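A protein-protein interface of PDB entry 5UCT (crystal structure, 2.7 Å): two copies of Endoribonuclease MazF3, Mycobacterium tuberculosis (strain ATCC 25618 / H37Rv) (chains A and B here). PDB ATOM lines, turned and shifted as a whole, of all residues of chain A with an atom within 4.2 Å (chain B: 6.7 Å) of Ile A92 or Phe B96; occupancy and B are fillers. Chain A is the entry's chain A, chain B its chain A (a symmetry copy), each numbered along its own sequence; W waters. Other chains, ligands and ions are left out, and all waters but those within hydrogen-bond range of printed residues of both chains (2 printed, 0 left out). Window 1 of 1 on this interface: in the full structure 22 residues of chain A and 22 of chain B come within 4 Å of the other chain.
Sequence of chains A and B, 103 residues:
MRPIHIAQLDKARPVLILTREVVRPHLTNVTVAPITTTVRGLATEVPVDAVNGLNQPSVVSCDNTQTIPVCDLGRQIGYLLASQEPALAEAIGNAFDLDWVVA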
ATOM      1  N   ARG A   2      21.725  17.805  16.049  1.00  0.00           N
ATOM      2  CA  ARG A   2      20.523  18.000  16.851  1.00  0.00           C
ATOM      3  C   ARG A   2      20.764  17.596  18.307  1.00  0.00           C
ATOM      4  O   ARG A   2      20.208  16.602  18.776  1.00  0.00           O
ATOM      5  CB  ARG A   2      19.365  17.194  16.260  1.00  0.00           C
ATOM      6  CG  ARG A   2      17.998  17.604  16.758  1.00  0.00           C
ATOM      7  CD  ARG A   2      17.607  18.974  16.230  1.00  0.00           C
ATOM      8  NE  ARG A   2      17.283  18.940  14.809  1.00  0.00           N
ATOM      9  CZ  ARG A   2      16.920  20.002  14.097  1.00  0.00           C
ATOM     10  NH1 ARG A   2      16.834  21.196  14.668  1.00  0.00           N
ATOM     11  NH2 ARG A   2      16.642  19.869  12.807  1.00  0.00           N
ATOM     12  N   LEU A  18      16.570  23.486  18.658  1.00  0.00           N
ATOM     13  CA  LEU A  18      15.862  23.605  17.390  1.00  0.00           C
ATOM     14  C   LEU A  18      16.668  24.395  16.370  1.00  0.00           C
ATOM     15  O   LEU A  18      16.652  24.066  15.178  1.00  0.00           O
ATOM     16  CB  LEU A  18      14.495  24.253  17.604  1.00  0.00           C
ATOM     17  CG  LEU A  18      13.450  23.377  18.286  1.00  0.00           C
ATOM     18  CD1 LEU A  18      12.094  24.051  18.238  1.00  0.00           C
ATOM     19  CD2 LEU A  18      13.397  22.006  17.626  1.00  0.00           C
ATOM     20  N   THR A  19      17.366  25.440  16.816  1.00  0.00           N
ATOM     21  CA  THR A  19      18.213  26.215  15.921  1.00  0.00           C
ATOM     22  C   THR A  19      19.220  25.309  15.226  1.00  0.00           C
ATOM     23  O   THR A  19      19.800  24.410  15.842  1.00  0.00           O
ATOM     24  CB  THR A  19      18.947  27.312  16.698  1.00  0.00           C
ATOM     25  OG1 THR A  19      17.997  28.114  17.410  1.00  0.00           O
ATOM     26  CG2 THR A  19      19.743  28.200  15.750  1.00  0.00           C
ATOM     27  N   THR A  31      17.034  28.769  19.683  1.00  0.00           N
ATOM     28  CA  THR A  31      15.663  28.301  19.820  1.00  0.00           C
ATOM     29  C   THR A  31      15.680  26.836  20.231  1.00  0.00           C
ATOM     30  O   THR A  31      16.354  26.016  19.601  1.00  0.00           O
ATOM     31  CB  THR A  31      14.886  28.480  18.515  1.00  0.00           C
ATOM     32  OG1 THR A  31      14.916  29.858  18.125  1.00  0.00           O
ATOM     33  CG2 THR A  31      13.440  28.049  18.690  1.00  0.00           C
ATOM     34  N   CYS A  62       6.874  20.263  21.353  1.00  0.00           N
ATOM     35  CA  CYS A  62       7.051  21.226  20.273  1.00  0.00           C
ATOM     36  C   CYS A  62       6.045  22.368  20.315  1.00  0.00           C
ATOM     37  O   CYS A  62       6.156  23.294  19.506  1.00  0.00           O
ATOM     38  CB  CYS A  62       6.961  20.521  18.920  1.00  0.00           C
ATOM     39  SG  CYS A  62       8.427  19.552  18.497  1.00  0.00           S
ATOM     40  N   LEU A  88      10.407  14.838  14.030  1.00  0.00           N
ATOM     41  CA  LEU A  88      10.565  16.210  14.508  1.00  0.00           C
ATOM     42  C   LEU A  88       9.961  17.203  13.526  1.00  0.00           C
ATOM     43  O   LEU A  88       9.184  18.086  13.915  1.00  0.00           O
ATOM     44  CB  LEU A  88      12.042  16.525  14.736  1.00  0.00           C
ATOM     45  CG  LEU A  88      12.338  18.006  14.985  1.00  0.00           C
ATOM     46  CD1 LEU A  88      11.716  18.463  16.295  1.00  0.00           C
ATOM     47  CD2 LEU A  88      13.835  18.281  14.965  1.00  0.00           C
ATOM     48  N   ALA A  89      10.318  17.083  12.246  1.00  0.00           N
ATOM     49  CA  ALA A  89       9.695  17.921  11.228  1.00  0.00           C
ATOM     50  C   ALA A  89       8.187  17.720  11.204  1.00  0.00           C
ATOM     51  O   ALA A  89       7.429  18.679  11.027  1.00  0.00           O
ATOM     52  CB  ALA A  89      10.297  17.621   9.856  1.00  0.00           C
ATOM     53  N   GLU A  90       7.731  16.480  11.393  1.00  0.00           N
ATOM     54  CA  GLU A  90       6.294  16.228  11.433  1.00  0.00           C
ATOM     55  C   GLU A  90       5.642  16.925  12.620  1.00  0.00           C
ATOM     56  O   GLU A  90       4.539  17.475  12.499  1.00  0.00           O
ATOM     57  CB  GLU A  90       6.026  14.723  11.486  1.00  0.00           C
ATOM     58  CG  GLU A  90       4.554  14.348  11.497  1.00  0.00           C
ATOM     59  CD  GLU A  90       3.890  14.526  10.145  1.00  0.00           C
ATOM     60  OE1 GLU A  90       4.561  14.986   9.198  1.00  0.00           O
ATOM     61  OE2 GLU A  90       2.692  14.198  10.030  1.00  0.00           O
ATOM     62  N   ALA A  91       6.308  16.913  13.777  1.00  0.00           N
ATOM     63  CA  ALA A  91       5.737  17.534  14.969  1.00  0.00           C
ATOM     64  C   ALA A  91       5.622  19.044  14.807  1.00  0.00           C
ATOM     65  O   ALA A  91       4.595  19.638  15.156  1.00  0.00           O
ATOM     66  CB  ALA A  91       6.580  17.189  16.194  1.00  0.00           C
ATOM     67  N   ILE A  92       6.666  19.683  14.273  1.00  0.00           N
ATOM     68  CA  ILE A  92       6.655  21.135  14.125  1.00  0.00           C
ATOM     69  C   ILE A  92       5.647  21.560  13.066  1.00  0.00           C
ATOM     70  O   ILE A  92       4.930  22.554  13.236  1.00  0.00           O
ATOM     71  CB  ILE A  92       8.073  21.647  13.806  1.00  0.00           C
ATOM     72  CG1 ILE A  92       8.992  21.464  15.016  1.00  0.00           C
ATOM     73  CG2 ILE A  92       8.037  23.108  13.380  1.00  0.00           C
ATOM     74  CD1 ILE A  92      10.421  21.909  14.778  1.00  0.00           C
ATOM     75  N   GLY A  93       5.566  20.812  11.964  1.00  0.00           N
ATOM     76  CA  GLY A  93       4.625  21.163  10.912  1.00  0.00           C
ATOM     77  C   GLY A  93       3.183  21.156  11.379  1.00  0.00           C
ATOM     78  O   GLY A  93       2.404  22.046  11.029  1.00  0.00           O
ATOM     79  N   ASN A  94       2.802  20.149  12.172  1.00  0.00           N
ATOM     80  CA  ASN A  94       1.448  20.126  12.713  1.00  0.00           C
ATOM     81  C   ASN A  94       1.276  21.157  13.817  1.00  0.00           C
ATOM     82  O   ASN A  94       0.189  21.723  13.970  1.00  0.00           O
ATOM     83  CB  ASN A  94       1.097  18.735  13.239  1.00  0.00           C
ATOM     84  CG  ASN A  94       1.296  17.654  12.205  1.00  0.00           C
ATOM     85  OD1 ASN A  94       0.943  17.827  11.042  1.00  0.00           O
ATOM     86  ND2 ASN A  94       1.869  16.528  12.621  1.00  0.00           N
ATOM     87  N   ALA A  95       2.334  21.419  14.589  1.00  0.00           N
ATOM     88  CA  ALA A  95       2.237  22.386  15.676  1.00  0.00           C
ATOM     89  C   ALA A  95       1.924  23.784  15.161  1.00  0.00           C
ATOM     90  O   ALA A  95       1.219  24.546  15.829  1.00  0.00           O
ATOM     91  CB  ALA A  95       3.530  22.404  16.489  1.00  0.00           C
ATOM     92  N   PHE A  96       2.428  24.134  13.979  1.00  0.00           N
ATOM     93  CA  PHE A  96       2.246  25.467  13.421  1.00  0.00           C
ATOM     94  C   PHE A  96       1.385  25.484  12.164  1.00  0.00           C
ATOM     95  O   PHE A  96       1.153  26.564  11.608  1.00  0.00           O
ATOM     96  CB  PHE A  96       3.613  26.101  13.121  1.00  0.00           C
ATOM     97  CG  PHE A  96       4.500  26.246  14.332  1.00  0.00           C
ATOM     98  CD1 PHE A  96       3.955  26.405  15.596  1.00  0.00           C
ATOM     99  CD2 PHE A  96       5.879  26.221  14.204  1.00  0.00           C
ATOM    100  CE1 PHE A  96       4.769  26.536  16.705  1.00  0.00           C
ATOM    101  CE2 PHE A  96       6.696  26.352  15.310  1.00  0.00           C
ATOM    102  CZ  PHE A  96       6.142  26.510  16.562  1.00  0.00           C
ATOM    103  N   LEU B  18       2.182  31.681  15.560  1.00  0.00           N
ATOM    104  CA  LEU B  18       2.669  30.458  14.934  1.00  0.00           C
ATOM    105  C   LEU B  18       1.782  29.267  15.267  1.00  0.00           C
ATOM    106  O   LEU B  18       1.559  28.403  14.411  1.00  0.00           O
ATOM    107  CB  LEU B  18       4.110  30.183  15.359  1.00  0.00           C
ATOM    108  CG  LEU B  18       5.164  31.101  14.750  1.00  0.00           C
ATOM    109  CD1 LEU B  18       6.552  30.588  15.074  1.00  0.00           C
ATOM    110  CD2 LEU B  18       4.964  31.211  13.245  1.00  0.00           C
ATOM    111  N   THR B  44      15.783  33.443   7.328  1.00  0.00           N
ATOM    112  CA  THR B  44      14.718  33.100   8.263  1.00  0.00           C
ATOM    113  C   THR B  44      13.759  34.255   8.517  1.00  0.00           C
ATOM    114  O   THR B  44      13.005  34.214   9.495  1.00  0.00           O
ATOM    115  CB  THR B  44      15.313  32.625   9.592  1.00  0.00           C
ATOM    116  OG1 THR B  44      15.921  33.734  10.270  1.00  0.00           O
ATOM    117  CG2 THR B  44      16.370  31.561   9.343  1.00  0.00           C
ATOM    118  N   CYS B  62      11.824  34.633  12.401  1.00  0.00           N
ATOM    119  CA  CYS B  62      11.561  33.241  12.744  1.00  0.00           C
ATOM    120  C   CYS B  62      12.668  32.608  13.575  1.00  0.00           C
ATOM    121  O   CYS B  62      12.513  31.460  14.005  1.00  0.00           O
ATOM    122  CB  CYS B  62      11.345  32.418  11.475  1.00  0.00           C
ATOM    123  SG  CYS B  62       9.738  32.684  10.691  1.00  0.00           S
ATOM    124  N   ASP B  63      13.780  33.305  13.801  1.00  0.00           N
ATOM    125  CA  ASP B  63      14.818  32.785  14.680  1.00  0.00           C
ATOM    126  C   ASP B  63      14.572  33.117  16.143  1.00  0.00           C
ATOM    127  O   ASP B  63      15.326  32.645  17.003  1.00  0.00           O
ATOM    128  CB  ASP B  63      16.186  33.326  14.259  1.00  0.00           C
ATOM    129  CG  ASP B  63      16.869  32.442  13.241  1.00  0.00           C
ATOM    130  OD1 ASP B  63      16.865  31.211  13.431  1.00  0.00           O
ATOM    131  OD2 ASP B  63      17.406  32.982  12.251  1.00  0.00           O
ATOM    132  N   THR B  65      11.346  32.840  17.793  1.00  0.00           N
ATOM    133  CA  THR B  65       9.999  32.432  18.168  1.00  0.00           C
ATOM    134  C   THR B  65       9.918  32.166  19.669  1.00  0.00           C
ATOM    135  O   THR B  65      10.873  31.692  20.292  1.00  0.00           O
ATOM    136  CB  THR B  65       9.577  31.181  17.398  1.00  0.00           C
ATOM    137  OG1 THR B  65      10.225  30.040  17.973  1.00  0.00           O
ATOM    138  CG2 THR B  65       9.973  31.301  15.930  1.00  0.00           C
ATOM    139  N   ALA B  91      10.736  29.719   5.797  1.00  0.00           N
ATOM    140  CA  ALA B  91      11.563  30.379   6.803  1.00  0.00           C
ATOM    141  C   ALA B  91      11.799  29.476   8.007  1.00  0.00           C
ATOM    142  O   ALA B  91      12.926  29.378   8.508  1.00  0.00           O
ATOM    143  CB  ALA B  91      10.913  31.690   7.237  1.00  0.00           C
ATOM    144  N   ILE B  92      10.749  28.803   8.482  1.00  0.00           N
ATOM    145  CA  ILE B  92      10.879  27.952   9.659  1.00  0.00           C
ATOM    146  C   ILE B  92      11.727  26.726   9.345  1.00  0.00           C
ATOM    147  O   ILE B  92      12.559  26.305  10.160  1.00  0.00           O
ATOM    148  CB  ILE B  92       9.486  27.564  10.192  1.00  0.00           C
ATOM    149  CG1 ILE B  92       8.776  28.790  10.771  1.00  0.00           C
ATOM    150  CG2 ILE B  92       9.596  26.466  11.242  1.00  0.00           C
ATOM    151  CD1 ILE B  92       7.380  28.507  11.288  1.00  0.00           C
ATOM    152  N   GLY B  93      11.542  26.141   8.161  1.00  0.00           N
ATOM    153  CA  GLY B  93      12.317  24.966   7.798  1.00  0.00           C
ATOM    154  C   GLY B  93      13.811  25.227   7.767  1.00  0.00           C
ATOM    155  O   GLY B  93      14.603  24.404   8.232  1.00  0.00           O
ATOM    156  N   ASN B  94      14.219  26.373   7.213  1.00  0.00           N
ATOM    157  CA  ASN B  94      15.637  26.714   7.218  1.00  0.00           C
ATOM    158  C   ASN B  94      16.099  27.135   8.604  1.00  0.00           C
ATOM    159  O   ASN B  94      17.248  26.875   8.977  1.00  0.00           O
ATOM    160  CB  ASN B  94      15.932  27.825   6.211  1.00  0.00           C
ATOM    161  CG  ASN B  94      15.450  27.493   4.820  1.00  0.00           C
ATOM    162  OD1 ASN B  94      15.613  26.370   4.352  1.00  0.00           O
ATOM    163  ND2 ASN B  94      14.848  28.470   4.147  1.00  0.00           N
ATOM    164  N   ALA B  95      15.222  27.775   9.381  1.00  0.00           N
ATOM    165  CA  ALA B  95      15.602  28.221  10.717  1.00  0.00           C
ATOM    166  C   ALA B  95      15.960  27.049  11.620  1.00  0.00           C
ATOM    167  O   ALA B  95      16.843  27.174  12.475  1.00  0.00           O
ATOM    168  CB  ALA B  95      14.476  29.042  11.344  1.00  0.00           C
ATOM    169  N   PHE B  96      15.298  25.907  11.444  1.00  0.00           N
ATOM    170  CA  PHE B  96      15.513  24.744  12.295  1.00  0.00           C
ATOM    171  C   PHE B  96      16.143  23.567  11.560  1.00  0.00           C
ATOM    172  O   PHE B  96      16.382  22.527  12.185  1.00  0.00           O
ATOM    173  CB  PHE B  96      14.187  24.308  12.933  1.00  0.00           C
ATOM    174  CG  PHE B  96      13.541  25.368  13.789  1.00  0.00           C
ATOM    175  CD1 PHE B  96      14.308  26.322  14.436  1.00  0.00           C
ATOM    176  CD2 PHE B  96      12.165  25.408  13.944  1.00  0.00           C
ATOM    177  CE1 PHE B  96      13.715  27.295  15.220  1.00  0.00           C
ATOM    178  CE2 PHE B  96      11.568  26.378  14.726  1.00  0.00           C
ATOM    179  CZ  PHE B  96      12.342  27.322  15.365  1.00  0.00           C
ATOM    180  N   ASP B  97      16.429  23.704  10.262  1.00  0.00           N
ATOM    181  CA  ASP B  97      16.946  22.617   9.425  1.00  0.00           C
ATOM    182  C   ASP B  97      16.015  21.401   9.480  1.00  0.00           C
ATOM    183  O   ASP B  97      16.313  20.363  10.075  1.00  0.00           O
ATOM    184  CB  ASP B  97      18.380  22.241   9.820  1.00  0.00           C
ATOM    185  CG  ASP B  97      19.413  23.194   9.249  1.00  0.00           C
ATOM    186  OD1 ASP B  97      19.018  24.202   8.624  1.00  0.00           O
ATOM    187  OD2 ASP B  97      20.621  22.936   9.427  1.00  0.00           O
ATOM    188  N   LEU B  98      14.866  21.571   8.835  1.00  0.00           N
ATOM    189  CA  LEU B  98      13.846  20.540   8.740  1.00  0.00           C
ATOM    190  C   LEU B  98      13.680  20.122   7.285  1.00  0.00           C
ATOM    191  O   LEU B  98      13.904  20.914   6.365  1.00  0.00           O
ATOM    192  CB  LEU B  98      12.510  21.035   9.304  1.00  0.00           C
ATOM    193  CG  LEU B  98      12.557  21.549  10.745  1.00  0.00           C
ATOM    194  CD1 LEU B  98      11.263  22.263  11.105  1.00  0.00           C
ATOM    195  CD2 LEU B  98      12.830  20.406  11.712  1.00  0.00           C
ATOM    196  N   TRP B 100      11.476  19.758   4.856  1.00  0.00           N
ATOM    197  CA  TRP B 100      10.201  20.104   4.235  1.00  0.00           C
ATOM    198  C   TRP B 100      10.152  19.608   2.795  1.00  0.00           C
ATOM    199  O   TRP B 100       9.469  20.189   1.953  1.00  0.00           O
ATOM    200  CB  TRP B 100       9.958  21.619   4.272  1.00  0.00           C
ATOM    201  CG  TRP B 100       9.306  22.193   5.534  1.00  0.00           C
ATOM    202  CD1 TRP B 100       9.197  23.520   5.846  1.00  0.00           C
ATOM    203  CD2 TRP B 100       8.674  21.480   6.621  1.00  0.00           C
ATOM    204  NE1 TRP B 100       8.552  23.679   7.046  1.00  0.00           N
ATOM    205  CE2 TRP B 100       8.221  22.447   7.543  1.00  0.00           C
ATOM    206  CE3 TRP B 100       8.452  20.127   6.907  1.00  0.00           C
ATOM    207  CZ2 TRP B 100       7.564  22.104   8.720  1.00  0.00           C
ATOM    208  CZ3 TRP B 100       7.800  19.793   8.078  1.00  0.00           C
ATOM    209  CH2 TRP B 100       7.366  20.778   8.967  1.00  0.00           C
HETATM  210  O   HOH W   1      13.037  30.309  16.245  1.00  0.00           O
HETATM  211  O   HOH W   2      17.214  30.244  16.159  1.00  0.00           O
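The backbone carbonyl oxygen (O) of Leu A18 sits close to the backbone carbonyl oxygen (O) of Phe B96 (3.4 Å).
The backbone carbonyl oxygen of Asp B97 sits at hydrogen-bond distance from the guanidinium group of Arg A2 (2.8 Å).
NH2 of Arg A2 sits at hydrogen-bond distance from O of Phe B96 (2.7 Å).
The side-chain hydroxyl of Thr A31 is in hydrogen-bond range of the backbone carbonyl oxygen of Asp B63 (3.0 Å).
O of Phe A96 lies close to O of Leu B18 (3.4 Å).
The guanidinium group (NH1) of Arg A2 lies within hydrogen-bond range of the backbone carbonyl oxygen (O) of Leu A18, at 2.9 Å.
The backbone NH (N) of Leu A18 is in hydrogen-bond range of the backbone carbonyl oxygen (O) of Thr A31 (2.7 Å).
The backbone NH (N) of Leu B98 sits at hydrogen-bond distance from the backbone carbonyl oxygen (O) of Gly B93 (2.9 Å).
The side-chain hydroxyl (OG1) of Thr A19 lies within hydrogen-bond range of the backbone NH (N) of Thr A31, 2.6 Å away.
OD2 of Asp B63 sits at hydrogen-bond distance from OG1 of Thr B44 (2.6 Å).
CA of Thr A19 touches O of Ala B95 (3.8 Å).
Thr A19 touches Phe B96 (N to CD1, 3.97 Å).
Thr A31 touches Thr B65 (CG2 to OG1, 3.8 Å).
CE1 of Phe B96 touches CG2 of Thr A31, at 3.6 Å.
CH2 of Trp B100 touches O of Ala A89 (2.9 Å).
Ile A92 touches Phe B96.
Ile A92 touches Leu B98 (CD1 to CD1, 3.8 Å).
Gly A93 touches Trp B100 (CA to CH2, 3.4 Å).
CD2 of Phe A96 touches CD1 of Ile B92, at 3.998 Å.
Of the printed residues of chain B, Ile A92 touches Phe B96 and Leu B98.
Printed residues of chain A within 4 Å of Phe B96: Arg A2 (2.7 Å), Leu A18 (3.2 Å), Thr A19 (3.97 Å), Thr A31 (3.6 Å) and Ile A92 (3.998 Å).
Printed residues of chain A within 4 Å of Leu B98: Ile A92 (3.8 Å).
Of the printed residues of chain B, Gly A93 touches Trp B100 (3.4 Å).
Ala B91 touches none of the printed residues of chain A.
Gly B93 touches none of the printed residues of chain A.
The nearest printed residue of chain B that does not touch Ile A92 is Ile B92 (4.3 Å).
Printed residues of chain B that touch a printed residue of chain A: Leu B18, Asp B63, Thr B65, Ile B92, Ala B95, Phe B96, Asp B97, Leu B98 and Trp B100.
Hydrophobic or aromatic side chains of chain B within 4 Å of the printed part of chain A: Leu B18, Ile B92, Phe B96, Leu B98 and Trp B100.
Among the printed residues, 14 pairs touch across the chains.
Among the printed residues, no Asp or Glu carboxylate lies within 4 Å of a Lys or Arg side-chain nitrogen of the other chain.
Leu A18 touches Phe B96, and with the chains exchanged Phe A96 touches Leu B18.
Ile A92 touches Phe B96, and with the chains exchanged Phe A96 touches Ile B92.
Of the 14 pairs that touch across the chains among the printed residues, 4 have their exchanged pair printed and touching as well.
Water W1 lies within hydrogen-bond range of O of Cys B62 (2.6 Å), OG1 of Thr A31 (2.7 Å), OG1 of Thr B65 (3.3 Å) and O of Asp B63 (3.4 Å).
Water W2 lies within hydrogen-bond range of OG1 of Thr A19 (2.6 Å), OD1 of Asp B63 (2.9 Å) and OG1 of Thr A31 (3.0 Å).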
